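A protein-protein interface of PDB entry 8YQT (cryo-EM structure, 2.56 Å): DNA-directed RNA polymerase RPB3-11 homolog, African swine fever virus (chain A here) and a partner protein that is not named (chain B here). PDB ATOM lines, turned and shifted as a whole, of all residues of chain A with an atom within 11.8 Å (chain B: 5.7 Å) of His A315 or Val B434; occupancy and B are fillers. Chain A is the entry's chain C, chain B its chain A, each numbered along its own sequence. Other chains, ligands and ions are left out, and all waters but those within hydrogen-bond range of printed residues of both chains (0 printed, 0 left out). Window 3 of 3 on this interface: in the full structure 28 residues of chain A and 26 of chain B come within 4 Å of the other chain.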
ATOM      1  N   ARG A 171      12.377 -15.478  36.103  1.00  0.00           N
ATOM      2  CA  ARG A 171      13.467 -15.325  35.152  1.00  0.00           C
ATOM      3  C   ARG A 171      13.016 -14.583  33.901  1.00  0.00           C
ATOM      4  O   ARG A 171      13.825 -13.908  33.255  1.00  0.00           O
ATOM      5  CB  ARG A 171      14.019 -16.705  34.805  1.00  0.00           C
ATOM      6  CG  ARG A 171      15.183 -16.710  33.861  1.00  0.00           C
ATOM      7  CD  ARG A 171      15.807 -18.082  33.832  1.00  0.00           C
ATOM      8  NE  ARG A 171      14.876 -19.104  33.369  1.00  0.00           N
ATOM      9  CZ  ARG A 171      14.764 -19.500  32.110  1.00  0.00           C
ATOM     10  NH1 ARG A 171      15.509 -18.975  31.152  1.00  0.00           N
ATOM     11  NH2 ARG A 171      13.885 -20.448  31.805  1.00  0.00           N
ATOM     12  N   THR A 282      23.451 -29.827  24.483  1.00  0.00           N
ATOM     13  CA  THR A 282      22.987 -28.458  24.294  1.00  0.00           C
ATOM     14  C   THR A 282      21.506 -28.407  24.640  1.00  0.00           C
ATOM     15  O   THR A 282      20.686 -29.048  23.975  1.00  0.00           O
ATOM     16  CB  THR A 282      23.231 -27.981  22.865  1.00  0.00           C
ATOM     17  OG1 THR A 282      24.621 -28.107  22.545  1.00  0.00           O
ATOM     18  CG2 THR A 282      22.818 -26.527  22.716  1.00  0.00           C
ATOM     19  N   ILE A 283      21.164 -27.651  25.678  1.00  0.00           N
ATOM     20  CA  ILE A 283      19.781 -27.490  26.105  1.00  0.00           C
ATOM     21  C   ILE A 283      19.401 -26.023  25.970  1.00  0.00           C
ATOM     22  O   ILE A 283      20.128 -25.134  26.438  1.00  0.00           O
ATOM     23  CB  ILE A 283      19.554 -27.991  27.541  1.00  0.00           C
ATOM     24  CG1 ILE A 283      20.279 -29.314  27.763  1.00  0.00           C
ATOM     25  CG2 ILE A 283      18.078 -28.212  27.778  1.00  0.00           C
ATOM     26  CD1 ILE A 283      19.710 -30.450  26.949  1.00  0.00           C
ATOM     27  N   LYS A 284      18.272 -25.781  25.314  1.00  0.00           N
ATOM     28  CA  LYS A 284      17.761 -24.437  25.115  1.00  0.00           C
ATOM     29  C   LYS A 284      17.071 -23.936  26.377  1.00  0.00           C
ATOM     30  O   LYS A 284      16.396 -24.689  27.083  1.00  0.00           O
ATOM     31  CB  LYS A 284      16.776 -24.415  23.947  1.00  0.00           C
ATOM     32  CG  LYS A 284      17.039 -23.341  22.909  1.00  0.00           C
ATOM     33  CD  LYS A 284      18.243 -23.681  22.049  1.00  0.00           C
ATOM     34  CE  LYS A 284      18.501 -22.598  21.013  1.00  0.00           C
ATOM     35  NZ  LYS A 284      18.594 -21.243  21.623  1.00  0.00           N
ATOM     36  N   ASP A 285      17.257 -22.645  26.656  1.00  0.00           N
ATOM     37  CA  ASP A 285      16.581 -21.962  27.759  1.00  0.00           C
ATOM     38  C   ASP A 285      16.955 -22.545  29.117  1.00  0.00           C
ATOM     39  O   ASP A 285      16.182 -22.464  30.072  1.00  0.00           O
ATOM     40  CB  ASP A 285      15.060 -21.982  27.576  1.00  0.00           C
ATOM     41  CG  ASP A 285      14.428 -20.628  27.809  1.00  0.00           C
ATOM     42  OD1 ASP A 285      13.234 -20.582  28.174  1.00  0.00           O
ATOM     43  OD2 ASP A 285      15.121 -19.606  27.622  1.00  0.00           O
ATOM     44  N   GLU A 286      18.138 -23.138  29.223  1.00  0.00           N
ATOM     45  CA  GLU A 286      18.640 -23.615  30.501  1.00  0.00           C
ATOM     46  C   GLU A 286      19.654 -22.635  31.065  1.00  0.00           C
ATOM     47  O   GLU A 286      20.268 -21.847  30.340  1.00  0.00           O
ATOM     48  CB  GLU A 286      19.261 -25.006  30.378  1.00  0.00           C
ATOM     49  CG  GLU A 286      18.248 -26.114  30.504  1.00  0.00           C
ATOM     50  CD  GLU A 286      17.569 -26.134  31.855  1.00  0.00           C
ATOM     51  OE1 GLU A 286      18.209 -25.736  32.848  1.00  0.00           O
ATOM     52  OE2 GLU A 286      16.394 -26.549  31.924  1.00  0.00           O
ATOM     53  N   THR A 287      19.818 -22.695  32.378  1.00  0.00           N
ATOM     54  CA  THR A 287      20.549 -21.696  33.135  1.00  0.00           C
ATOM     55  C   THR A 287      21.695 -22.351  33.895  1.00  0.00           C
ATOM     56  O   THR A 287      21.948 -23.551  33.778  1.00  0.00           O
ATOM     57  CB  THR A 287      19.609 -20.961  34.092  1.00  0.00           C
ATOM     58  OG1 THR A 287      19.034 -21.897  35.009  1.00  0.00           O
ATOM     59  CG2 THR A 287      18.497 -20.296  33.316  1.00  0.00           C
ATOM     60  N   HIS A 288      22.392 -21.532  34.684  1.00  0.00           N
ATOM     61  CA  HIS A 288      23.541 -22.005  35.441  1.00  0.00           C
ATOM     62  C   HIS A 288      23.158 -22.992  36.534  1.00  0.00           C
ATOM     63  O   HIS A 288      24.025 -23.730  37.003  1.00  0.00           O
ATOM     64  CB  HIS A 288      24.283 -20.820  36.051  1.00  0.00           C
ATOM     65  CG  HIS A 288      24.889 -19.904  35.037  1.00  0.00           C
ATOM     66  ND1 HIS A 288      26.148 -20.101  34.516  1.00  0.00           N
ATOM     67  CD2 HIS A 288      24.404 -18.792  34.441  1.00  0.00           C
ATOM     68  CE1 HIS A 288      26.415 -19.145  33.646  1.00  0.00           C
ATOM     69  NE2 HIS A 288      25.372 -18.337  33.582  1.00  0.00           N
ATOM     70  N   GLN A 311      29.139 -24.214  29.701  1.00  0.00           N
ATOM     71  CA  GLN A 311      29.012 -22.830  29.247  1.00  0.00           C
ATOM     72  C   GLN A 311      27.559 -22.440  28.975  1.00  0.00           C
ATOM     73  O   GLN A 311      26.890 -23.042  28.136  1.00  0.00           O
ATOM     74  CB  GLN A 311      29.856 -22.628  27.991  1.00  0.00           C
ATOM     75  CG  GLN A 311      29.995 -21.186  27.566  1.00  0.00           C
ATOM     76  CD  GLN A 311      30.819 -21.034  26.307  1.00  0.00           C
ATOM     77  OE1 GLN A 311      31.161 -22.018  25.654  1.00  0.00           O
ATOM     78  NE2 GLN A 311      31.147 -19.798  25.961  1.00  0.00           N
ATOM     79  N   CYS A 312      27.069 -21.429  29.694  1.00  0.00           N
ATOM     80  CA  CYS A 312      25.751 -20.842  29.459  1.00  0.00           C
ATOM     81  C   CYS A 312      25.971 -19.451  28.891  1.00  0.00           C
ATOM     82  O   CYS A 312      26.457 -18.563  29.596  1.00  0.00           O
ATOM     83  CB  CYS A 312      24.926 -20.758  30.742  1.00  0.00           C
ATOM     84  SG  CYS A 312      24.495 -22.316  31.501  1.00  0.00           S
ATOM     85  N   VAL A 313      25.607 -19.244  27.635  1.00  0.00           N
ATOM     86  CA  VAL A 313      25.964 -18.012  26.926  1.00  0.00           C
ATOM     87  C   VAL A 313      24.758 -17.078  26.904  1.00  0.00           C
ATOM     88  O   VAL A 313      23.678 -17.497  26.467  1.00  0.00           O
ATOM     89  CB  VAL A 313      26.477 -18.282  25.501  1.00  0.00           C
ATOM     90  CG1 VAL A 313      26.652 -16.971  24.762  1.00  0.00           C
ATOM     91  CG2 VAL A 313      27.800 -19.014  25.558  1.00  0.00           C
ATOM     92  N   PRO A 314      24.895 -15.833  27.373  1.00  0.00           N
ATOM     93  CA  PRO A 314      23.720 -14.954  27.482  1.00  0.00           C
ATOM     94  C   PRO A 314      23.034 -14.648  26.162  1.00  0.00           C
ATOM     95  O   PRO A 314      21.799 -14.610  26.126  1.00  0.00           O
ATOM     96  CB  PRO A 314      24.296 -13.681  28.119  1.00  0.00           C
ATOM     97  CG  PRO A 314      25.534 -14.124  28.799  1.00  0.00           C
ATOM     98  CD  PRO A 314      26.100 -15.208  27.940  1.00  0.00           C
ATOM     99  N   HIS A 315      23.778 -14.433  25.081  1.00  0.00           N
ATOM    100  CA  HIS A 315      23.160 -14.077  23.810  1.00  0.00           C
ATOM    101  C   HIS A 315      22.769 -15.290  22.984  1.00  0.00           C
ATOM    102  O   HIS A 315      22.261 -15.126  21.871  1.00  0.00           O
ATOM    103  CB  HIS A 315      24.082 -13.161  22.992  1.00  0.00           C
ATOM    104  CG  HIS A 315      25.278 -13.848  22.408  1.00  0.00           C
ATOM    105  ND1 HIS A 315      25.224 -14.568  21.236  1.00  0.00           N
ATOM    106  CD2 HIS A 315      26.567 -13.894  22.816  1.00  0.00           C
ATOM    107  CE1 HIS A 315      26.423 -15.046  20.959  1.00  0.00           C
ATOM    108  NE2 HIS A 315      27.257 -14.649  21.901  1.00  0.00           N
ATOM    109  N   LYS A 316      22.985 -16.497  23.499  1.00  0.00           N
ATOM    110  CA  LYS A 316      22.590 -17.715  22.815  1.00  0.00           C
ATOM    111  C   LYS A 316      21.413 -18.418  23.470  1.00  0.00           C
ATOM    112  O   LYS A 316      20.809 -19.288  22.836  1.00  0.00           O
ATOM    113  CB  LYS A 316      23.777 -18.683  22.732  1.00  0.00           C
ATOM    114  CG  LYS A 316      24.917 -18.169  21.878  1.00  0.00           C
ATOM    115  CD  LYS A 316      26.023 -19.193  21.755  1.00  0.00           C
ATOM    116  CE  LYS A 316      25.622 -20.319  20.828  1.00  0.00           C
ATOM    117  NZ  LYS A 316      25.410 -19.832  19.441  1.00  0.00           N
ATOM    118  N   GLN A 317      21.071 -18.059  24.708  1.00  0.00           N
ATOM    119  CA  GLN A 317      19.986 -18.700  25.453  1.00  0.00           C
ATOM    120  C   GLN A 317      20.185 -20.211  25.531  1.00  0.00           C
ATOM    121  O   GLN A 317      19.234 -20.990  25.450  1.00  0.00           O
ATOM    122  CB  GLN A 317      18.623 -18.362  24.848  1.00  0.00           C
ATOM    123  CG  GLN A 317      18.079 -16.993  25.226  1.00  0.00           C
ATOM    124  CD  GLN A 317      18.156 -15.988  24.092  1.00  0.00           C
ATOM    125  OE1 GLN A 317      18.333 -16.353  22.930  1.00  0.00           O
ATOM    126  NE2 GLN A 317      18.012 -14.714  24.426  1.00  0.00           N
ATOM    127  N   GLU A 318      21.437 -20.630  25.697  1.00  0.00           N
ATOM    128  CA  GLU A 318      21.783 -22.041  25.682  1.00  0.00           C
ATOM    129  C   GLU A 318      22.729 -22.386  26.819  1.00  0.00           C
ATOM    130  O   GLU A 318      23.638 -21.606  27.157  1.00  0.00           O
ATOM    131  CB  GLU A 318      22.448 -22.454  24.365  1.00  0.00           C
ATOM    132  CG  GLU A 318      21.520 -22.588  23.186  1.00  0.00           C
ATOM    133  CD  GLU A 318      22.273 -22.917  21.916  1.00  0.00           C
ATOM    134  OE1 GLU A 318      23.521 -22.924  21.957  1.00  0.00           O
ATOM    135  OE2 GLU A 318      21.626 -23.164  20.879  1.00  0.00           O
ATOM    136  N   MET A 319      22.508 -23.578  27.380  1.00  0.00           N
ATOM    137  CA  MET A 319      23.482 -24.269  28.215  1.00  0.00           C
ATOM    138  C   MET A 319      24.115 -25.384  27.394  1.00  0.00           C
ATOM    139  O   MET A 319      23.409 -26.250  26.869  1.00  0.00           O
ATOM    140  CB  MET A 319      22.820 -24.851  29.467  1.00  0.00           C
ATOM    141  CG  MET A 319      23.779 -25.478  30.474  1.00  0.00           C
ATOM    142  SD  MET A 319      24.163 -27.215  30.188  1.00  0.00           S
ATOM    143  CE  MET A 319      22.643 -28.003  30.692  1.00  0.00           C
ATOM    144  N   VAL A 320      25.440 -25.366  27.285  1.00  0.00           N
ATOM    145  CA  VAL A 320      26.188 -26.378  26.553  1.00  0.00           C
ATOM    146  C   VAL A 320      27.157 -27.034  27.522  1.00  0.00           C
ATOM    147  O   VAL A 320      28.086 -26.385  28.020  1.00  0.00           O
ATOM    148  CB  VAL A 320      26.932 -25.783  25.347  1.00  0.00           C
ATOM    149  CG1 VAL A 320      27.591 -26.881  24.542  1.00  0.00           C
ATOM    150  CG2 VAL A 320      25.980 -24.992  24.481  1.00  0.00           C
ATOM    151  N   ASN B 330      30.564  -7.037  24.245  1.00  0.00           N
ATOM    152  CA  ASN B 330      30.179  -8.438  24.363  1.00  0.00           C
ATOM    153  C   ASN B 330      31.449  -9.272  24.359  1.00  0.00           C
ATOM    154  O   ASN B 330      32.137  -9.352  23.339  1.00  0.00           O
ATOM    155  CB  ASN B 330      29.243  -8.847  23.224  1.00  0.00           C
ATOM    156  CG  ASN B 330      28.596 -10.194  23.449  1.00  0.00           C
ATOM    157  OD1 ASN B 330      29.130 -11.042  24.153  1.00  0.00           O
ATOM    158  ND2 ASN B 330      27.428 -10.392  22.860  1.00  0.00           N
ATOM    159  N   ASP B 332      31.730 -12.514  24.751  1.00  0.00           N
ATOM    160  CA  ASP B 332      31.574 -13.840  24.172  1.00  0.00           C
ATOM    161  C   ASP B 332      31.784 -13.858  22.669  1.00  0.00           C
ATOM    162  O   ASP B 332      31.823 -14.943  22.078  1.00  0.00           O
ATOM    163  CB  ASP B 332      30.186 -14.397  24.489  1.00  0.00           C
ATOM    164  CG  ASP B 332      30.044 -14.800  25.932  1.00  0.00           C
ATOM    165  OD1 ASP B 332      31.024 -15.320  26.507  1.00  0.00           O
ATOM    166  OD2 ASP B 332      28.955 -14.583  26.497  1.00  0.00           O
ATOM    167  N   LEU B 333      31.911 -12.697  22.039  1.00  0.00           N
ATOM    168  CA  LEU B 333      32.161 -12.632  20.610  1.00  0.00           C
ATOM    169  C   LEU B 333      33.654 -12.648  20.336  1.00  0.00           C
ATOM    170  O   LEU B 333      34.445 -12.092  21.100  1.00  0.00           O
ATOM    171  CB  LEU B 333      31.543 -11.371  20.014  1.00  0.00           C
ATOM    172  CG  LEU B 333      30.027 -11.237  20.088  1.00  0.00           C
ATOM    173  CD1 LEU B 333      29.617  -9.868  19.616  1.00  0.00           C
ATOM    174  CD2 LEU B 333      29.347 -12.314  19.273  1.00  0.00           C
ATOM    175  N   GLU B 337      34.186 -11.042  14.967  1.00  0.00           N
ATOM    176  CA  GLU B 337      32.745 -11.225  14.941  1.00  0.00           C
ATOM    177  C   GLU B 337      32.055  -9.950  15.393  1.00  0.00           C
ATOM    178  O   GLU B 337      32.589  -9.199  16.213  1.00  0.00           O
ATOM    179  CB  GLU B 337      32.312 -12.387  15.833  1.00  0.00           C
ATOM    180  CG  GLU B 337      32.609 -13.751  15.262  1.00  0.00           C
ATOM    181  CD  GLU B 337      32.300 -14.863  16.237  1.00  0.00           C
ATOM    182  OE1 GLU B 337      32.054 -14.563  17.422  1.00  0.00           O
ATOM    183  OE2 GLU B 337      32.302 -16.041  15.822  1.00  0.00           O
ATOM    184  N   VAL B 338      30.868  -9.707  14.851  1.00  0.00           N
ATOM    185  CA  VAL B 338      30.012  -8.611  15.279  1.00  0.00           C
ATOM    186  C   VAL B 338      28.638  -9.181  15.597  1.00  0.00           C
ATOM    187  O   VAL B 338      28.104  -9.998  14.841  1.00  0.00           O
ATOM    188  CB  VAL B 338      29.931  -7.488  14.218  1.00  0.00           C
ATOM    189  CG1 VAL B 338      29.393  -8.009  12.894  1.00  0.00           C
ATOM    190  CG2 VAL B 338      29.094  -6.329  14.721  1.00  0.00           C
ATOM    191  N   GLY B 339      28.086  -8.784  16.741  1.00  0.00           N
ATOM    192  CA  GLY B 339      26.749  -9.191  17.120  1.00  0.00           C
ATOM    193  C   GLY B 339      25.726  -8.332  16.411  1.00  0.00           C
ATOM    194  O   GLY B 339      25.777  -7.102  16.481  1.00  0.00           O
ATOM    195  N   TYR B 340      24.791  -8.985  15.729  1.00  0.00           N
ATOM    196  CA  TYR B 340      23.867  -8.298  14.846  1.00  0.00           C
ATOM    197  C   TYR B 340      22.436  -8.622  15.257  1.00  0.00           C
ATOM    198  O   TYR B 340      22.065  -9.803  15.325  1.00  0.00           O
ATOM    199  CB  TYR B 340      24.128  -8.705  13.391  1.00  0.00           C
ATOM    200  CG  TYR B 340      23.611  -7.724  12.370  1.00  0.00           C
ATOM    201  CD1 TYR B 340      23.851  -6.367  12.503  1.00  0.00           C
ATOM    202  CD2 TYR B 340      22.903  -8.157  11.261  1.00  0.00           C
ATOM    203  CE1 TYR B 340      23.386  -5.470  11.576  1.00  0.00           C
ATOM    204  CE2 TYR B 340      22.438  -7.264  10.325  1.00  0.00           C
ATOM    205  CZ  TYR B 340      22.685  -5.922  10.488  1.00  0.00           C
ATOM    206  OH  TYR B 340      22.224  -5.022   9.562  1.00  0.00           O
ATOM    207  N   PRO B 341      21.613  -7.618  15.549  1.00  0.00           N
ATOM    208  CA  PRO B 341      20.227  -7.889  15.942  1.00  0.00           C
ATOM    209  C   PRO B 341      19.453  -8.602  14.845  1.00  0.00           C
ATOM    210  O   PRO B 341      19.660  -8.372  13.653  1.00  0.00           O
ATOM    211  CB  PRO B 341      19.655  -6.491  16.203  1.00  0.00           C
ATOM    212  CG  PRO B 341      20.839  -5.640  16.463  1.00  0.00           C
ATOM    213  CD  PRO B 341      21.932  -6.184  15.608  1.00  0.00           C
ATOM    214  N   THR B 411      24.141 -16.233  10.617  1.00  0.00           N
ATOM    215  CA  THR B 411      25.434 -16.307  11.279  1.00  0.00           C
ATOM    216  C   THR B 411      26.477 -16.872  10.324  1.00  0.00           C
ATOM    217  O   THR B 411      26.237 -17.874   9.644  1.00  0.00           O
ATOM    218  CB  THR B 411      25.337 -17.164  12.540  1.00  0.00           C
ATOM    219  OG1 THR B 411      24.463 -16.534  13.481  1.00  0.00           O
ATOM    220  CG2 THR B 411      26.700 -17.341  13.180  1.00  0.00           C
ATOM    221  N   GLY B 412      27.639 -16.228  10.277  1.00  0.00           N
ATOM    222  CA  GLY B 412      28.709 -16.610   9.379  1.00  0.00           C
ATOM    223  C   GLY B 412      28.850 -15.718   8.169  1.00  0.00           C
ATOM    224  O   GLY B 412      29.886 -15.779   7.498  1.00  0.00           O
ATOM    225  N   ARG B 432      32.638 -11.407  10.897  1.00  0.00           N
ATOM    226  CA  ARG B 432      31.669 -12.478  10.731  1.00  0.00           C
ATOM    227  C   ARG B 432      30.456 -12.199  11.602  1.00  0.00           C
ATOM    228  O   ARG B 432      30.585 -11.889  12.786  1.00  0.00           O
ATOM    229  CB  ARG B 432      32.282 -13.828  11.090  1.00  0.00           C
ATOM    230  CG  ARG B 432      33.397 -14.251  10.164  1.00  0.00           C
ATOM    231  CD  ARG B 432      34.008 -15.562  10.605  1.00  0.00           C
ATOM    232  NE  ARG B 432      34.742 -15.421  11.855  1.00  0.00           N
ATOM    233  CZ  ARG B 432      34.448 -16.068  12.972  1.00  0.00           C
ATOM    234  NH1 ARG B 432      33.436 -16.919  13.032  1.00  0.00           N
ATOM    235  NH2 ARG B 432      35.186 -15.859  14.058  1.00  0.00           N
ATOM    236  N   ILE B 433      29.279 -12.302  11.007  1.00  0.00           N
ATOM    237  CA  ILE B 433      28.048 -11.916  11.683  1.00  0.00           C
ATOM    238  C   ILE B 433      27.616 -13.018  12.638  1.00  0.00           C
ATOM    239  O   ILE B 433      27.613 -14.200  12.283  1.00  0.00           O
ATOM    240  CB  ILE B 433      26.948 -11.606  10.658  1.00  0.00           C
ATOM    241  CG1 ILE B 433      27.218 -10.258  10.001  1.00  0.00           C
ATOM    242  CG2 ILE B 433      25.582 -11.619  11.310  1.00  0.00           C
ATOM    243  CD1 ILE B 433      26.468 -10.065   8.738  1.00  0.00           C
ATOM    244  N   VAL B 434      27.274 -12.630  13.863  1.00  0.00           N
ATOM    245  CA  VAL B 434      26.545 -13.476  14.798  1.00  0.00           C
ATOM    246  C   VAL B 434      25.196 -12.815  15.031  1.00  0.00           C
ATOM    247  O   VAL B 434      25.129 -11.699  15.559  1.00  0.00           O
ATOM    248  CB  VAL B 434      27.306 -13.663  16.118  1.00  0.00           C
ATOM    249  CG1 VAL B 434      26.535 -14.578  17.046  1.00  0.00           C
ATOM    250  CG2 VAL B 434      28.689 -14.211  15.859  1.00  0.00           C
ATOM    251  N   VAL B 435      24.125 -13.488  14.631  1.00  0.00           N
ATOM    252  CA  VAL B 435      22.790 -12.909  14.730  1.00  0.00           C
ATOM    253  C   VAL B 435      22.252 -13.122  16.136  1.00  0.00           C
ATOM    254  O   VAL B 435      22.233 -14.249  16.643  1.00  0.00           O
ATOM    255  CB  VAL B 435      21.852 -13.512  13.672  1.00  0.00           C
ATOM    256  CG1 VAL B 435      20.446 -12.969  13.842  1.00  0.00           C
ATOM    257  CG2 VAL B 435      22.366 -13.202  12.284  1.00  0.00           C
ATOM    258  N   LEU B 436      21.817 -12.037  16.770  1.00  0.00           N
ATOM    259  CA  LEU B 436      21.314 -12.072  18.137  1.00  0.00           C
ATOM    260  C   LEU B 436      19.819 -12.368  18.093  1.00  0.00           C
ATOM    261  O   LEU B 436      19.024 -11.525  17.671  1.00  0.00           O
ATOM    262  CB  LEU B 436      21.602 -10.751  18.846  1.00  0.00           C
ATOM    263  CG  LEU B 436      23.043 -10.242  18.761  1.00  0.00           C
ATOM    264  CD1 LEU B 436      23.169  -8.856  19.364  1.00  0.00           C
ATOM    265  CD2 LEU B 436      24.009 -11.205  19.425  1.00  0.00           C
ATOM    266  N   GLU B 437      19.440 -13.565  18.537  1.00  0.00           N
ATOM    267  CA  GLU B 437      18.055 -14.006  18.445  1.00  0.00           C
ATOM    268  C   GLU B 437      17.138 -13.304  19.434  1.00  0.00           C
ATOM    269  O   GLU B 437      15.916 -13.358  19.265  1.00  0.00           O
ATOM    270  CB  GLU B 437      17.973 -15.515  18.665  1.00  0.00           C
ATOM    271  CG  GLU B 437      18.912 -16.323  17.792  1.00  0.00           C
ATOM    272  CD  GLU B 437      18.508 -16.316  16.337  1.00  0.00           C
ATOM    273  OE1 GLU B 437      17.296 -16.235  16.058  1.00  0.00           O
ATOM    274  OE2 GLU B 437      19.404 -16.394  15.473  1.00  0.00           O
ATOM    275  N   ASN B 438      17.688 -12.666  20.457  1.00  0.00           N
ATOM    276  CA  ASN B 438      16.879 -11.934  21.423  1.00  0.00           C
ATOM    277  C   ASN B 438      16.227 -10.741  20.737  1.00  0.00           C
ATOM    278  O   ASN B 438      16.940  -9.884  20.201  1.00  0.00           O
ATOM    279  CB  ASN B 438      17.752 -11.475  22.585  1.00  0.00           C
ATOM    280  CG  ASN B 438      16.947 -11.006  23.780  1.00  0.00           C
ATOM    281  OD1 ASN B 438      15.720 -11.068  23.784  1.00  0.00           O
ATOM    282  ND2 ASN B 438      17.640 -10.529  24.803  1.00  0.00           N
ATOM    283  N   ILE B 441      17.140  -6.617  21.689  1.00  0.00           N
ATOM    284  CA  ILE B 441      18.493  -6.091  21.557  1.00  0.00           C
ATOM    285  C   ILE B 441      18.582  -5.348  20.234  1.00  0.00           C
ATOM    286  O   ILE B 441      18.322  -5.926  19.173  1.00  0.00           O
ATOM    287  CB  ILE B 441      19.547  -7.205  21.637  1.00  0.00           C
ATOM    288  CG1 ILE B 441      19.582  -7.793  23.044  1.00  0.00           C
ATOM    289  CG2 ILE B 441      20.913  -6.671  21.262  1.00  0.00           C
ATOM    290  CD1 ILE B 441      20.477  -8.990  23.170  1.00  0.00           C
ATOM    291  N   GLN B 445      26.988  -5.391  18.683  1.00  0.00           N
ATOM    292  CA  GLN B 445      27.819  -5.865  19.773  1.00  0.00           C
ATOM    293  C   GLN B 445      29.127  -6.408  19.222  1.00  0.00           C
ATOM    294  O   GLN B 445      29.149  -7.061  18.177  1.00  0.00           O
ATOM    295  CB  GLN B 445      27.085  -6.928  20.586  1.00  0.00           C
ATOM    296  CG  GLN B 445      25.797  -6.404  21.174  1.00  0.00           C
ATOM    297  CD  GLN B 445      25.149  -7.365  22.132  1.00  0.00           C
ATOM    298  OE1 GLN B 445      25.651  -8.460  22.366  1.00  0.00           O
ATOM    299  NE2 GLN B 445      24.023  -6.960  22.697  1.00  0.00           N
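Among the printed residues, merely in contact across the chains: Val A313 with Asp B332 (3.7 Å), Pro A314 with Asp B332 (3.3 Å), His A315 with Asn B330 (3.6 Å), His A315 with Asp B332 (3.9 Å), His A315 with Val B434 (3.9 Å) and Gln A317 with Asn B438 (3.7 Å).
Printed residues of chain B within 4 Å of His A315: Asn B330 (3.6 Å), Asp B332 (3.9 Å) and Val B434 (3.9 Å).
Val B434 touches one residue of chain A.
Asp B332 touches just these residues of chain A: Val A313, Pro A314 and His A315.
No residue of chain A comes within 4 Å of Leu B333.
No residue of chain A comes within 4 Å of Glu B337.
No residue of chain A comes within 4 Å of Pro B341.
Thr B411 touches none of the printed residues of chain A.
No residue of chain A comes within 4 Å of Gly B412.
No residue of chain A comes within 4 Å of Ile B433.
No residue of chain A comes within 4 Å of Gln B445.
Printed residues of chain B within 4 Å of Val A313: Asp B332 (3.7 Å).
Of the printed residues of chain A, Asn B438 touches Gln A317.
Of the printed residues of chain B, Gln A317 touches Asn B438.
Of the printed residues of chain A, Asn B330 touches His A315.
His A288 touches none of the printed residues of chain B.
The nearest residue of chain A that does not touch Val B434 is Lys A316 (5.9 Å).
The nearest printed residue of chain B that does not touch Val A313 is Asn B330 (6.5 Å).
The backbone NH (N) of Asp B332 is in hydrogen-bond range of the side-chain amide oxygen (OD1) of Asn B330.
The side-chain amide oxygen (OE1) of Gln B445 is in hydrogen-bond range of the side-chain amide nitrogen (ND2) of Asn B330 (2.7 Å).
The backbone NH (N) of Val B434 lies within hydrogen-bond range of the backbone carbonyl oxygen (O) of Val B338, at 2.9 Å.
O of Val B434 sits at hydrogen-bond distance from N of Tyr B340, 2.7 Å away.
The backbone NH (N) of Asp A285 lies within hydrogen-bond range of the backbone carbonyl oxygen (O) of Gln A317 (2.8 Å).
The backbone NH (N) of Val A313 sits at hydrogen-bond distance from the backbone carbonyl oxygen (O) of Glu A318.
Of the 19 printed residues of chain B, 4 touch a printed residue of chain A.
Hydrophobic or aromatic side chains of chain B that line the printed part of chain A: Val B434.
Printed residues of chain A that touch a printed residue of chain B: Val A313, Pro A314, His A315 and Gln A317.
Hydrophobic or aromatic side chains of chain A within 4 Å of the printed part of chain B: Val A313, Pro A314 and His A315.
Among the printed residues, no Asp or Glu carboxylate lies within 4 Å of a Lys or Arg side-chain nitrogen of the other chain.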
